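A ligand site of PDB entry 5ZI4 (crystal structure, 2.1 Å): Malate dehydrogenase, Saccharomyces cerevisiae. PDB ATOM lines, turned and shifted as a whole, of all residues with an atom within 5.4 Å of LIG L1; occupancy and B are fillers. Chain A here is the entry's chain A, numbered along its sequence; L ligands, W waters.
Water W1 lies within hydrogen-bond range of an oxygen (O8) of LIG L1 (2.6 Å), the backbone NH of Gly 16 (2.9 Å), the backbone carbonyl oxygen of Pro 77 (3.3 Å), the backbone carbonyl oxygen of Gly 10 (3.3 Å) and the backbone NH of Val 15 (3.4 Å). Water W6 lies within hydrogen-bond range of the side-chain hydroxyl of Ser 234 (2.5 Å), the backbone carbonyl oxygen of Ala 235 (2.6 Å) and an oxygen (O9) of LIG L1 (2.6 Å). Water W8 lies within hydrogen-bond range of an oxygen (O2) of LG2 L2 (2.6 Å), an oxygen (O13) of LIG L1 (2.7 Å), the side-chain hydroxyl (OG) of Ser 234 (2.8 Å) and the backbone NH (N) of Arg 82 (2.9 Å). Water W3 bridges the guanidinium group of Arg 38 and an oxygen (O5) of LIG L1. Water W5 bridges O9 of LIG L1 (2.8 Å) and N of Ser 234 (3.1 Å). Water W4 lies within hydrogen-bond range of the side-chain hydroxyl of Ser 101 (2.8 Å) and a nitrogen (N3) of LIG L1 (2.9 Å).
O4 of LIG L1 sits at hydrogen-bond distance from N of Gly 79. The side-chain carboxylate (OD1) of Asp 36 sits at hydrogen-bond distance from an oxygen (O6) of LIG L1, at 2.4 Å. The backbone NH (N) of Val 15 sits at hydrogen-bond distance from an oxygen (O8) of LIG L1, 2.8 Å away. An oxygen (O5) of LG2 L2 sits at hydrogen-bond distance from the side-chain amide nitrogen (ND2) of Asn 120, 3.2 Å away. O5 of LG2 L2 is in hydrogen-bond range of NE2 of His 189. N of Gly 13 lies within hydrogen-bond range of O5 of LIG L1 (3.1 Å). The backbone carbonyl oxygen (O) of Val 80 is in hydrogen-bond range of an oxygen (O12) of LIG L1, at 3.2 Å. O of Val 147 lies within hydrogen-bond range of N7 of LIG L1 (3.2 Å). NE2 of His 189 is in hydrogen-bond range of O14 of LIG L1, at 2.8 Å. A nitrogen (N7) of LIG L1 sits at hydrogen-bond distance from the backbone carbonyl oxygen (O) of Ile 118 (3.0 Å). The backbone NH of Gly 14 lies within hydrogen-bond range of an oxygen (O1) of LIG L1 (2.8 Å). NH1 of Arg 82 lies within salt-bridge range of O1 of LG2 L2, at 2.6 Å. The side-chain amide oxygen (OD1) of Asn 95 sits at hydrogen-bond distance from an oxygen (O12) of LIG L1, at 3.3 Å. The backbone NH of Asn 120 lies within hydrogen-bond range of an oxygen (O12) of LIG L1, 3.3 Å away.
SD of Met 239 sits close to O14 of LIG L1, 3.4 Å away. Gly 10 touches LIG L1. Ser 12 touches LIG L1. CE2 of Tyr 35 touches C9 of LIG L1, at 3.4 Å. Ile 37 touches LIG L1. Pro 77 touches LIG L1 (O to C11, 3.0 Å). Ala 78 touches LIG L1 (CA to O4, 3.4 Å). Pro 81 touches LIG L1. Ile 98 touches LIG L1. CD2 of Leu 102 touches N4 of LIG L1, 3.5 Å away. Ser 119 touches LIG L1. CG2 of Val 122 touches N7 of LIG L1, at 3.7 Å. O of Ala 235 touches C20 of LIG L1, 3.3 Å away. CG2 of Thr 236 touches O9 of LIG L1, 3.7 Å away. 25 residues have an atom within 4 Å of LIG L1: Gly 10, Ser 12, Gly 13, Gly 14, Val 15, Tyr 35, Asp 36, Ile 37, Pro 77, Ala 78, Gly 79, Val 80, Pro 81, Asn 95, Ile 98, Leu 102, Ile 118, Ser 119, Asn 120, Val 122, Val 147, His 189, Ala 235, Thr 236 and Met 239. The nearest printed residue that does not touch LIG L1 is Leu 150 (4.1 Å).
ND2 of Asn 95 lies close to O of Asn 120 (3.4 Å). O of Ala 78 sits at hydrogen-bond distance from OG of Ser 119 (2.7 Å). The side-chain carboxylate (OD2) of Asp 36 lies within hydrogen-bond range of the backbone NH (N) of Ala 11. The backbone carbonyl oxygen of Leu 9 is in hydrogen-bond range of the backbone NH of Ala 78 (3.0 Å). The side-chain amide oxygen of Asn 95 lies within hydrogen-bond range of the backbone NH of Val 80 (2.8 Å). The backbone carbonyl oxygen (O) of Tyr 35 is in hydrogen-bond range of the backbone NH (N) of Ala 11 (3.1 Å). N of Val 147 lies within hydrogen-bond range of O of Val 117 (2.8 Å). The backbone NH (N) of Ser 12 is in hydrogen-bond range of the side-chain carboxylate (OD2) of Asp 36 (3.0 Å).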
ATOM      1  N   LEU A   9     -28.174 -25.535  18.084  1.00  0.00           N
ATOM      2  CA  LEU A   9     -28.191 -24.076  18.297  1.00  0.00           C
ATOM      3  C   LEU A   9     -26.740 -23.699  18.654  1.00  0.00           C
ATOM      4  O   LEU A   9     -26.235 -24.095  19.684  1.00  0.00           O
ATOM      5  CB  LEU A   9     -29.204 -23.709  19.405  1.00  0.00           C
ATOM      6  CG  LEU A   9     -30.585 -24.370  19.200  1.00  0.00           C
ATOM      7  CD1 LEU A   9     -31.534 -24.022  20.325  1.00  0.00           C
ATOM      8  CD2 LEU A   9     -31.237 -24.022  17.868  1.00  0.00           C
ATOM      9  N   GLY A  10     -26.072 -22.974  17.756  1.00  0.00           N
ATOM     10  CA  GLY A  10     -24.647 -22.720  17.876  1.00  0.00           C
ATOM     11  C   GLY A  10     -23.788 -23.568  16.939  1.00  0.00           C
ATOM     12  O   GLY A  10     -22.621 -23.780  17.204  1.00  0.00           O
ATOM     13  N   ALA A  11     -24.364 -23.986  15.809  1.00  0.00           N
ATOM     14  CA  ALA A  11     -23.764 -24.962  14.913  1.00  0.00           C
ATOM     15  C   ALA A  11     -22.538 -24.507  14.131  1.00  0.00           C
ATOM     16  O   ALA A  11     -21.958 -25.292  13.433  1.00  0.00           O
ATOM     17  CB  ALA A  11     -24.818 -25.449  13.933  1.00  0.00           C
ATOM     18  N   SER A  12     -22.170 -23.234  14.209  1.00  0.00           N
ATOM     19  CA  SER A  12     -21.095 -22.735  13.372  1.00  0.00           C
ATOM     20  C   SER A  12     -19.824 -22.518  14.188  1.00  0.00           C
ATOM     21  O   SER A  12     -18.856 -22.066  13.669  1.00  0.00           O
ATOM     22  CB  SER A  12     -21.518 -21.416  12.713  1.00  0.00           C
ATOM     23  OG  SER A  12     -22.739 -21.555  11.957  1.00  0.00           O
ATOM     24  N   GLY A  13     -19.833 -22.873  15.438  1.00  0.00           N
ATOM     25  CA  GLY A  13     -18.725 -22.621  16.299  1.00  0.00           C
ATOM     26  C   GLY A  13     -17.707 -23.726  16.243  1.00  0.00           C
ATOM     27  O   GLY A  13     -17.854 -24.651  15.449  1.00  0.00           O
ATOM     28  N   GLY A  14     -16.675 -23.607  17.100  1.00  0.00           N
ATOM     29  CA  GLY A  14     -15.558 -24.569  17.143  1.00  0.00           C
ATOM     30  C   GLY A  14     -16.119 -25.950  17.470  1.00  0.00           C
ATOM     31  O   GLY A  14     -15.780 -26.952  16.834  1.00  0.00           O
ATOM     32  N   VAL A  15     -17.018 -25.996  18.434  1.00  0.00           N
ATOM     33  CA  VAL A  15     -17.662 -27.261  18.813  1.00  0.00           C
ATOM     34  C   VAL A  15     -18.780 -27.606  17.833  1.00  0.00           C
ATOM     35  O   VAL A  15     -18.910 -28.720  17.429  1.00  0.00           O
ATOM     36  CB  VAL A  15     -18.219 -27.173  20.248  1.00  0.00           C
ATOM     37  CG1 VAL A  15     -18.981 -28.425  20.597  1.00  0.00           C
ATOM     38  CG2 VAL A  15     -17.071 -26.931  21.231  1.00  0.00           C
ATOM     39  N   GLY A  16     -19.536 -26.594  17.401  1.00  0.00           N
ATOM     40  CA  GLY A  16     -20.770 -26.796  16.662  1.00  0.00           C
ATOM     41  C   GLY A  16     -20.578 -27.390  15.263  1.00  0.00           C
ATOM     42  O   GLY A  16     -21.406 -28.240  14.852  1.00  0.00           O
ATOM     43  N   TYR A  35     -28.513 -23.937  13.370  1.00  0.00           N
ATOM     44  CA  TYR A  35     -28.812 -22.522  13.659  1.00  0.00           C
ATOM     45  C   TYR A  35     -27.632 -21.884  14.379  1.00  0.00           C
ATOM     46  O   TYR A  35     -27.063 -22.485  15.298  1.00  0.00           O
ATOM     47  CB  TYR A  35     -30.069 -22.421  14.513  1.00  0.00           C
ATOM     48  CG  TYR A  35     -30.339 -21.073  15.007  1.00  0.00           C
ATOM     49  CD1 TYR A  35     -30.945 -20.134  14.193  1.00  0.00           C
ATOM     50  CD2 TYR A  35     -29.884 -20.677  16.287  1.00  0.00           C
ATOM     51  CE1 TYR A  35     -31.164 -18.827  14.649  1.00  0.00           C
ATOM     52  CE2 TYR A  35     -30.069 -19.369  16.727  1.00  0.00           C
ATOM     53  CZ  TYR A  35     -30.711 -18.450  15.917  1.00  0.00           C
ATOM     54  OH  TYR A  35     -30.871 -17.158  16.352  1.00  0.00           O
ATOM     55  N   ASP A  36     -27.295 -20.671  13.958  1.00  0.00           N
ATOM     56  CA  ASP A  36     -26.277 -19.870  14.598  1.00  0.00           C
ATOM     57  C   ASP A  36     -26.583 -18.382  14.309  1.00  0.00           C
ATOM     58  O   ASP A  36     -27.457 -18.070  13.490  1.00  0.00           O
ATOM     59  CB  ASP A  36     -24.872 -20.315  14.139  1.00  0.00           C
ATOM     60  CG  ASP A  36     -23.748 -19.888  15.123  1.00  0.00           C
ATOM     61  OD1 ASP A  36     -23.439 -18.684  15.253  1.00  0.00           O
ATOM     62  OD2 ASP A  36     -23.084 -20.769  15.712  1.00  0.00           O
ATOM     63  N   ILE A  37     -25.943 -17.489  15.063  1.00  0.00           N
ATOM     64  CA  ILE A  37     -26.013 -16.102  14.777  1.00  0.00           C
ATOM     65  C   ILE A  37     -25.379 -15.818  13.421  1.00  0.00           C
ATOM     66  O   ILE A  37     -25.667 -14.814  12.850  1.00  0.00           O
ATOM     67  CB  ILE A  37     -25.361 -15.198  15.828  1.00  0.00           C
ATOM     68  CG1 ILE A  37     -24.006 -15.659  16.234  1.00  0.00           C
ATOM     69  CG2 ILE A  37     -26.196 -15.080  17.087  1.00  0.00           C
ATOM     70  CD1 ILE A  37     -23.391 -14.752  17.337  1.00  0.00           C
ATOM     71  N   ARG A  38     -24.526 -16.702  12.914  1.00  0.00           N
ATOM     72  CA  ARG A  38     -23.894 -16.524  11.600  1.00  0.00           C
ATOM     73  C   ARG A  38     -23.561 -17.864  10.958  1.00  0.00           C
ATOM     74  O   ARG A  38     -23.270 -18.866  11.675  1.00  0.00           O
ATOM     75  CB  ARG A  38     -22.544 -15.765  11.751  1.00  0.00           C
ATOM     76  CG  ARG A  38     -21.568 -16.339  12.814  1.00  0.00           C
ATOM     77  CD  ARG A  38     -20.185 -15.665  12.849  1.00  0.00           C
ATOM     78  NE  ARG A  38     -19.514 -15.952  11.568  1.00  0.00           N
ATOM     79  CZ  ARG A  38     -18.918 -17.121  11.222  1.00  0.00           C
ATOM     80  NH1 ARG A  38     -18.769 -18.141  12.087  1.00  0.00           N
ATOM     81  NH2 ARG A  38     -18.411 -17.250  10.002  1.00  0.00           N
ATOM     82  N   PRO A  77     -24.513 -26.238  21.624  1.00  0.00           N
ATOM     83  CA  PRO A  77     -23.119 -25.855  21.709  1.00  0.00           C
ATOM     84  C   PRO A  77     -22.843 -24.356  21.654  1.00  0.00           C
ATOM     85  O   PRO A  77     -21.699 -23.970  21.684  1.00  0.00           O
ATOM     86  CB  PRO A  77     -22.513 -26.513  20.485  1.00  0.00           C
ATOM     87  CG  PRO A  77     -23.621 -26.509  19.494  1.00  0.00           C
ATOM     88  CD  PRO A  77     -24.826 -26.815  20.314  1.00  0.00           C
ATOM     89  N   ALA A  78     -23.860 -23.543  21.506  1.00  0.00           N
ATOM     90  CA  ALA A  78     -23.701 -22.106  21.494  1.00  0.00           C
ATOM     91  C   ALA A  78     -23.088 -21.649  22.823  1.00  0.00           C
ATOM     92  O   ALA A  78     -23.343 -22.233  23.888  1.00  0.00           O
ATOM     93  CB  ALA A  78     -25.081 -21.429  21.240  1.00  0.00           C
ATOM     94  N   GLY A  79     -22.229 -20.652  22.734  1.00  0.00           N
ATOM     95  CA  GLY A  79     -21.578 -20.132  23.907  1.00  0.00           C
ATOM     96  C   GLY A  79     -20.405 -19.294  23.588  1.00  0.00           C
ATOM     97  O   GLY A  79     -20.049 -19.122  22.447  1.00  0.00           O
ATOM     98  N   VAL A  80     -19.831 -18.704  24.619  1.00  0.00           N
ATOM     99  CA  VAL A  80     -18.528 -18.103  24.542  1.00  0.00           C
ATOM    100  C   VAL A  80     -17.575 -19.050  25.300  1.00  0.00           C
ATOM    101  O   VAL A  80     -17.859 -19.443  26.440  1.00  0.00           O
ATOM    102  CB  VAL A  80     -18.559 -16.683  25.159  1.00  0.00           C
ATOM    103  CG1 VAL A  80     -17.154 -16.115  25.229  1.00  0.00           C
ATOM    104  CG2 VAL A  80     -19.395 -15.764  24.280  1.00  0.00           C
ATOM    105  N   PRO A  81     -16.460 -19.429  24.672  1.00  0.00           N
ATOM    106  CA  PRO A  81     -15.498 -20.253  25.363  1.00  0.00           C
ATOM    107  C   PRO A  81     -14.524 -19.442  26.262  1.00  0.00           C
ATOM    108  O   PRO A  81     -14.551 -18.187  26.288  1.00  0.00           O
ATOM    109  CB  PRO A  81     -14.744 -20.929  24.221  1.00  0.00           C
ATOM    110  CG  PRO A  81     -14.676 -19.847  23.192  1.00  0.00           C
ATOM    111  CD  PRO A  81     -16.035 -19.178  23.285  1.00  0.00           C
ATOM    112  N   ARG A  82     -13.679 -20.173  26.972  1.00  0.00           N
ATOM    113  CA  ARG A  82     -12.577 -19.549  27.713  1.00  0.00           C
ATOM    114  C   ARG A  82     -11.624 -18.774  26.804  1.00  0.00           C
ATOM    115  O   ARG A  82     -11.383 -19.167  25.672  1.00  0.00           O
ATOM    116  CB  ARG A  82     -11.789 -20.586  28.485  1.00  0.00           C
ATOM    117  CG  ARG A  82     -12.425 -20.906  29.830  1.00  0.00           C
ATOM    118  CD  ARG A  82     -11.414 -21.568  30.740  1.00  0.00           C
ATOM    119  NE  ARG A  82     -11.700 -22.977  31.016  1.00  0.00           N
ATOM    120  CZ  ARG A  82     -10.764 -23.871  31.347  1.00  0.00           C
ATOM    121  NH1 ARG A  82     -11.101 -25.129  31.596  1.00  0.00           N
ATOM    122  NH2 ARG A  82      -9.470 -23.542  31.411  1.00  0.00           N
ATOM    123  N   LYS A  83     -11.104 -17.667  27.316  1.00  0.00           N
ATOM    124  CA  LYS A  83     -10.254 -16.743  26.570  1.00  0.00           C
ATOM    125  C   LYS A  83      -9.264 -16.129  27.531  1.00  0.00           C
ATOM    126  O   LYS A  83      -9.618 -15.920  28.704  1.00  0.00           O
ATOM    127  CB  LYS A  83     -11.105 -15.600  25.993  1.00  0.00           C
ATOM    128  CG  LYS A  83     -10.750 -15.134  24.578  1.00  0.00           C
ATOM    129  CD  LYS A  83     -11.990 -14.738  23.776  1.00  0.00           C
ATOM    130  CE  LYS A  83     -13.031 -15.863  23.793  1.00  0.00           C
ATOM    131  NZ  LYS A  83     -13.830 -16.003  22.557  1.00  0.00           N
ATOM    132  N   ASN A  95     -22.684 -16.404  28.679  1.00  0.00           N
ATOM    133  CA  ASN A  95     -23.242 -17.716  28.367  1.00  0.00           C
ATOM    134  C   ASN A  95     -24.613 -17.852  28.989  1.00  0.00           C
ATOM    135  O   ASN A  95     -25.517 -18.452  28.380  1.00  0.00           O
ATOM    136  CB  ASN A  95     -22.296 -18.835  28.837  1.00  0.00           C
ATOM    137  CG  ASN A  95     -21.116 -19.061  27.876  1.00  0.00           C
ATOM    138  OD1 ASN A  95     -21.263 -19.679  26.829  1.00  0.00           O
ATOM    139  ND2 ASN A  95     -19.963 -18.608  28.249  1.00  0.00           N
ATOM    140  N   ILE A  98     -27.103 -16.243  26.618  1.00  0.00           N
ATOM    141  CA  ILE A  98     -27.228 -17.104  25.438  1.00  0.00           C
ATOM    142  C   ILE A  98     -28.080 -18.335  25.755  1.00  0.00           C
ATOM    143  O   ILE A  98     -28.971 -18.713  24.950  1.00  0.00           O
ATOM    144  CB  ILE A  98     -25.825 -17.510  24.895  1.00  0.00           C
ATOM    145  CG1 ILE A  98     -25.104 -16.272  24.302  1.00  0.00           C
ATOM    146  CG2 ILE A  98     -25.943 -18.663  23.884  1.00  0.00           C
ATOM    147  CD1 ILE A  98     -23.611 -16.477  24.059  1.00  0.00           C
ATOM    148  N   SER A 101     -31.824 -17.212  26.413  1.00  0.00           N
ATOM    149  CA  SER A 101     -32.396 -16.805  25.171  1.00  0.00           C
ATOM    150  C   SER A 101     -32.770 -18.022  24.253  1.00  0.00           C
ATOM    151  O   SER A 101     -33.874 -18.098  23.717  1.00  0.00           O
ATOM    152  CB  SER A 101     -31.389 -15.887  24.445  1.00  0.00           C
ATOM    153  OG  SER A 101     -31.807 -15.721  23.125  1.00  0.00           O
ATOM    154  N   LEU A 102     -31.843 -18.975  24.079  1.00  0.00           N
ATOM    155  CA  LEU A 102     -32.089 -20.139  23.211  1.00  0.00           C
ATOM    156  C   LEU A 102     -33.064 -21.097  23.860  1.00  0.00           C
ATOM    157  O   LEU A 102     -33.919 -21.695  23.179  1.00  0.00           O
ATOM    158  CB  LEU A 102     -30.740 -20.845  22.927  1.00  0.00           C
ATOM    159  CG  LEU A 102     -29.808 -19.976  22.093  1.00  0.00           C
ATOM    160  CD1 LEU A 102     -28.470 -20.610  21.958  1.00  0.00           C
ATOM    161  CD2 LEU A 102     -30.470 -19.743  20.724  1.00  0.00           C
ATOM    162  N   VAL A 117     -27.492 -29.550  26.769  1.00  0.00           N
ATOM    163  CA  VAL A 117     -26.733 -28.332  26.997  1.00  0.00           C
ATOM    164  C   VAL A 117     -25.255 -28.652  27.027  1.00  0.00           C
ATOM    165  O   VAL A 117     -24.779 -29.392  27.874  1.00  0.00           O
ATOM    166  CB  VAL A 117     -27.172 -27.632  28.321  1.00  0.00           C
ATOM    167  CG1 VAL A 117     -26.392 -26.327  28.476  1.00  0.00           C
ATOM    168  CG2 VAL A 117     -28.672 -27.361  28.280  1.00  0.00           C
ATOM    169  N   ILE A 118     -24.522 -28.122  26.060  1.00  0.00           N
ATOM    170  CA  ILE A 118     -23.078 -28.288  26.009  1.00  0.00           C
ATOM    171  C   ILE A 118     -22.396 -27.034  26.552  1.00  0.00           C
ATOM    172  O   ILE A 118     -21.282 -27.087  27.011  1.00  0.00           O
ATOM    173  CB  ILE A 118     -22.648 -28.582  24.561  1.00  0.00           C
ATOM    174  CG1 ILE A 118     -23.162 -29.956  24.113  1.00  0.00           C
ATOM    175  CG2 ILE A 118     -21.154 -28.525  24.444  1.00  0.00           C
ATOM    176  CD1 ILE A 118     -23.285 -30.164  22.642  1.00  0.00           C
ATOM    177  N   SER A 119     -23.042 -25.883  26.421  1.00  0.00           N
ATOM    178  CA  SER A 119     -22.517 -24.602  26.862  1.00  0.00           C
ATOM    179  C   SER A 119     -21.923 -24.682  28.239  1.00  0.00           C
ATOM    180  O   SER A 119     -22.465 -25.364  29.072  1.00  0.00           O
ATOM    181  CB  SER A 119     -23.664 -23.604  26.859  1.00  0.00           C
ATOM    182  OG  SER A 119     -24.515 -23.813  25.724  1.00  0.00           O
ATOM    183  N   ASN A 120     -20.871 -23.914  28.508  1.00  0.00           N
ATOM    184  CA  ASN A 120     -20.199 -23.953  29.831  1.00  0.00           C
ATOM    185  C   ASN A 120     -20.273 -22.568  30.536  1.00  0.00           C
ATOM    186  O   ASN A 120     -20.190 -21.575  29.850  1.00  0.00           O
ATOM    187  CB  ASN A 120     -18.768 -24.422  29.603  1.00  0.00           C
ATOM    188  CG  ASN A 120     -18.254 -25.330  30.679  1.00  0.00           C
ATOM    189  OD1 ASN A 120     -18.957 -26.208  31.200  1.00  0.00           O
ATOM    190  ND2 ASN A 120     -17.013 -25.124  31.027  1.00  0.00           N
ATOM    191  N   VAL A 122     -21.586 -25.599  32.534  1.00  0.00           N
ATOM    192  CA  VAL A 122     -22.699 -26.546  32.645  1.00  0.00           C
ATOM    193  C   VAL A 122     -23.392 -26.506  34.031  1.00  0.00           C
ATOM    194  O   VAL A 122     -24.610 -26.516  34.096  1.00  0.00           O
ATOM    195  CB  VAL A 122     -22.198 -27.992  32.382  1.00  0.00           C
ATOM    196  CG1 VAL A 122     -23.297 -29.042  32.610  1.00  0.00           C
ATOM    197  CG2 VAL A 122     -21.696 -28.106  30.942  1.00  0.00           C
ATOM    198  N   VAL A 147     -24.569 -31.930  29.122  1.00  0.00           N
ATOM    199  CA  VAL A 147     -23.691 -32.963  28.493  1.00  0.00           C
ATOM    200  C   VAL A 147     -22.346 -32.888  29.166  1.00  0.00           C
ATOM    201  O   VAL A 147     -21.571 -31.869  29.001  1.00  0.00           O
ATOM    202  CB  VAL A 147     -23.553 -32.799  26.975  1.00  0.00           C
ATOM    203  CG1 VAL A 147     -22.741 -33.925  26.394  1.00  0.00           C
ATOM    204  CG2 VAL A 147     -24.939 -32.732  26.296  1.00  0.00           C
ATOM    205  N   LEU A 150     -17.849 -35.611  27.921  1.00  0.00           N
ATOM    206  CA  LEU A 150     -16.427 -35.421  27.654  1.00  0.00           C
ATOM    207  C   LEU A 150     -15.569 -35.808  28.866  1.00  0.00           C
ATOM    208  O   LEU A 150     -14.423 -36.151  28.747  1.00  0.00           O
ATOM    209  CB  LEU A 150     -16.126 -34.025  27.171  1.00  0.00           C
ATOM    210  CG  LEU A 150     -14.670 -33.764  26.836  1.00  0.00           C
ATOM    211  CD1 LEU A 150     -14.236 -34.716  25.737  1.00  0.00           C
ATOM    212  CD2 LEU A 150     -14.454 -32.291  26.476  1.00  0.00           C
ATOM    213  N   HIS A 189     -19.197 -30.590  36.030  1.00  0.00           N
ATOM    214  CA  HIS A 189     -18.237 -30.351  34.971  1.00  0.00           C
ATOM    215  C   HIS A 189     -17.370 -29.150  35.320  1.00  0.00           C
ATOM    216  O   HIS A 189     -17.606 -28.031  34.892  1.00  0.00           O
ATOM    217  CB  HIS A 189     -19.006 -30.064  33.682  1.00  0.00           C
ATOM    218  CG  HIS A 189     -18.124 -30.070  32.479  1.00  0.00           C
ATOM    219  ND1 HIS A 189     -17.667 -31.244  31.919  1.00  0.00           N
ATOM    220  CD2 HIS A 189     -17.536 -29.068  31.805  1.00  0.00           C
ATOM    221  CE1 HIS A 189     -16.847 -30.961  30.927  1.00  0.00           C
ATOM    222  NE2 HIS A 189     -16.757 -29.640  30.828  1.00  0.00           N
ATOM    223  N   SER A 234     -10.398 -23.553  23.325  1.00  0.00           N
ATOM    224  CA  SER A 234     -10.514 -24.651  24.214  1.00  0.00           C
ATOM    225  C   SER A 234     -10.874 -25.889  23.382  1.00  0.00           C
ATOM    226  O   SER A 234     -10.906 -25.847  22.169  1.00  0.00           O
ATOM    227  CB  SER A 234     -11.607 -24.353  25.262  1.00  0.00           C
ATOM    228  OG  SER A 234     -12.736 -23.708  24.699  1.00  0.00           O
ATOM    229  N   ALA A 235     -11.093 -26.995  24.063  1.00  0.00           N
ATOM    230  CA  ALA A 235     -11.472 -28.244  23.435  1.00  0.00           C
ATOM    231  C   ALA A 235     -12.689 -28.025  22.529  1.00  0.00           C
ATOM    232  O   ALA A 235     -13.691 -27.463  22.984  1.00  0.00           O
ATOM    233  CB  ALA A 235     -11.841 -29.264  24.518  1.00  0.00           C
ATOM    234  N   THR A 236     -12.590 -28.511  21.296  1.00  0.00           N
ATOM    235  CA  THR A 236     -13.657 -28.416  20.264  1.00  0.00           C
ATOM    236  C   THR A 236     -13.981 -29.770  19.656  1.00  0.00           C
ATOM    237  O   THR A 236     -15.102 -30.239  19.724  1.00  0.00           O
ATOM    238  CB  THR A 236     -13.240 -27.456  19.131  1.00  0.00           C
ATOM    239  OG1 THR A 236     -11.950 -27.807  18.633  1.00  0.00           O
ATOM    240  CG2 THR A 236     -13.213 -26.004  19.613  1.00  0.00           C
ATOM    241  N   MET A 239     -14.794 -32.488  22.140  1.00  0.00           N
ATOM    242  CA  MET A 239     -16.151 -32.164  22.570  1.00  0.00           C
ATOM    243  C   MET A 239     -17.197 -32.577  21.565  1.00  0.00           C
ATOM    244  O   MET A 239     -18.198 -33.114  21.941  1.00  0.00           O
ATOM    245  CB  MET A 239     -16.351 -30.682  22.959  1.00  0.00           C
ATOM    246  CG  MET A 239     -17.783 -30.386  23.403  1.00  0.00           C
ATOM    247  SD  MET A 239     -18.124 -31.224  24.987  1.00  0.00           S
ATOM    248  CE  MET A 239     -19.617 -32.121  24.623  1.00  0.00           C
HETATM  249  P1  LIG L   1     -16.962 -20.689  19.561  1.00  0.00           P
HETATM  250  O1  LIG L   1     -16.022 -21.381  18.631  1.00  0.00           O
HETATM  251  O2  LIG L   1     -16.886 -19.313  20.127  1.00  0.00           O
HETATM  252  O3  LIG L   1     -18.476 -21.066  19.190  1.00  0.00           O
HETATM  253  C1  LIG L   1     -19.570 -20.365  19.697  1.00  0.00           C
HETATM  254  C2  LIG L   1     -20.716 -20.408  18.670  1.00  0.00           C
HETATM  255  O4  LIG L   1     -21.893 -20.080  19.407  1.00  0.00           O
HETATM  256  C3  LIG L   1     -20.489 -19.403  17.522  1.00  0.00           C
HETATM  257  O5  LIG L   1     -20.776 -19.973  16.197  1.00  0.00           O
HETATM  258  C4  LIG L   1     -21.479 -18.364  17.974  1.00  0.00           C
HETATM  259  O6  LIG L   1     -21.986 -17.633  16.922  1.00  0.00           O
HETATM  260  C5  LIG L   1     -22.603 -19.162  18.628  1.00  0.00           C
HETATM  261  N1  LIG L   1     -23.592 -18.373  19.392  1.00  0.00           N
HETATM  262  C6  LIG L   1     -23.432 -17.441  20.373  1.00  0.00           C
HETATM  263  N2  LIG L   1     -24.647 -16.950  20.771  1.00  0.00           N
HETATM  264  C7  LIG L   1     -25.590 -17.549  20.010  1.00  0.00           C
HETATM  265  C8  LIG L   1     -27.041 -17.501  19.914  1.00  0.00           C
HETATM  266  N3  LIG L   1     -27.661 -16.674  20.713  1.00  0.00           N
HETATM  267  N4  LIG L   1     -27.721 -18.278  19.055  1.00  0.00           N
HETATM  268  C9  LIG L   1     -27.013 -19.099  18.255  1.00  0.00           C
HETATM  269  N5  LIG L   1     -25.661 -19.210  18.301  1.00  0.00           N
HETATM  270  C10 LIG L   1     -24.917 -18.472  19.127  1.00  0.00           C
HETATM  271  O7  LIG L   1     -16.956 -21.585  20.925  1.00  0.00           O
HETATM  272  P2  LIG L   1     -16.779 -23.153  21.123  1.00  0.00           P
HETATM  273  O8  LIG L   1     -17.584 -23.859  20.112  1.00  0.00           O
HETATM  274  O9  LIG L   1     -15.317 -23.487  21.320  1.00  0.00           O
HETATM  275  O10 LIG L   1     -17.431 -23.299  22.549  1.00  0.00           O
HETATM  276  C11 LIG L   1     -18.852 -23.480  22.654  1.00  0.00           C
HETATM  277  C12 LIG L   1     -19.293 -23.663  24.104  1.00  0.00           C
HETATM  278  O11 LIG L   1     -19.115 -25.044  24.502  1.00  0.00           O
HETATM  279  C13 LIG L   1     -18.492 -22.795  25.106  1.00  0.00           C
HETATM  280  O12 LIG L   1     -19.408 -22.244  26.076  1.00  0.00           O
HETATM  281  C14 LIG L   1     -17.519 -23.822  25.662  1.00  0.00           C
HETATM  282  O13 LIG L   1     -16.919 -23.605  26.925  1.00  0.00           O
HETATM  283  C15 LIG L   1     -18.391 -25.054  25.736  1.00  0.00           C
HETATM  284  N6  LIG L   1     -17.664 -26.330  25.904  1.00  0.00           N
HETATM  285  C16 LIG L   1     -18.241 -27.238  26.697  1.00  0.00           C
HETATM  286  C17 LIG L   1     -17.672 -28.473  26.915  1.00  0.00           C
HETATM  287  C18 LIG L   1     -18.327 -29.479  27.833  1.00  0.00           C
HETATM  288  O14 LIG L   1     -17.615 -30.376  28.279  1.00  0.00           O
HETATM  289  N7  LIG L   1     -19.650 -29.412  28.114  1.00  0.00           N
HETATM  290  C19 LIG L   1     -16.476 -28.780  26.266  1.00  0.00           C
HETATM  291  C20 LIG L   1     -15.880 -27.868  25.432  1.00  0.00           C
HETATM  292  C21 LIG L   1     -16.497 -26.631  25.277  1.00  0.00           C
HETATM  293  O1  LG2 L   2     -12.600 -26.098  29.644  1.00  0.00           O
HETATM  294  O2  LG2 L   2     -13.323 -24.152  28.992  1.00  0.00           O
HETATM  295  O3  LG2 L   2     -13.933 -29.445  29.446  1.00  0.00           O
HETATM  296  O4  LG2 L   2     -12.877 -28.729  27.710  1.00  0.00           O
HETATM  297  O5  LG2 L   2     -15.768 -27.490  29.182  1.00  0.00           O
HETATM  298  C1  LG2 L   2     -13.315 -25.390  28.926  1.00  0.00           C
HETATM  299  C2  LG2 L   2     -14.264 -26.093  27.979  1.00  0.00           C
HETATM  300  C3  LG2 L   2     -14.673 -27.401  28.612  1.00  0.00           C
HETATM  301  C4  LG2 L   2     -13.766 -28.569  28.576  1.00  0.00           C
HETATM  302  O   HOH W   1     -19.862 -24.143  18.991  1.00  0.00           O
HETATM  303  O   HOH W   2     -18.929 -32.903  28.017  1.00  0.00           O
HETATM  304  O   HOH W   3     -19.252 -18.380  14.653  1.00  0.00           O
HETATM  305  O   HOH W   4     -30.495 -16.104  20.711  1.00  0.00           O
HETATM  306  O   HOH W   5     -12.616 -22.736  21.258  1.00  0.00           O
HETATM  307  O   HOH W   6     -14.420 -24.998  23.296  1.00  0.00           O
HETATM  308  O   HOH W   7     -15.738 -20.084  16.264  1.00  0.00           O
HETATM  309  O   HOH W   8     -14.300 -23.011  26.915  1.00  0.00           O
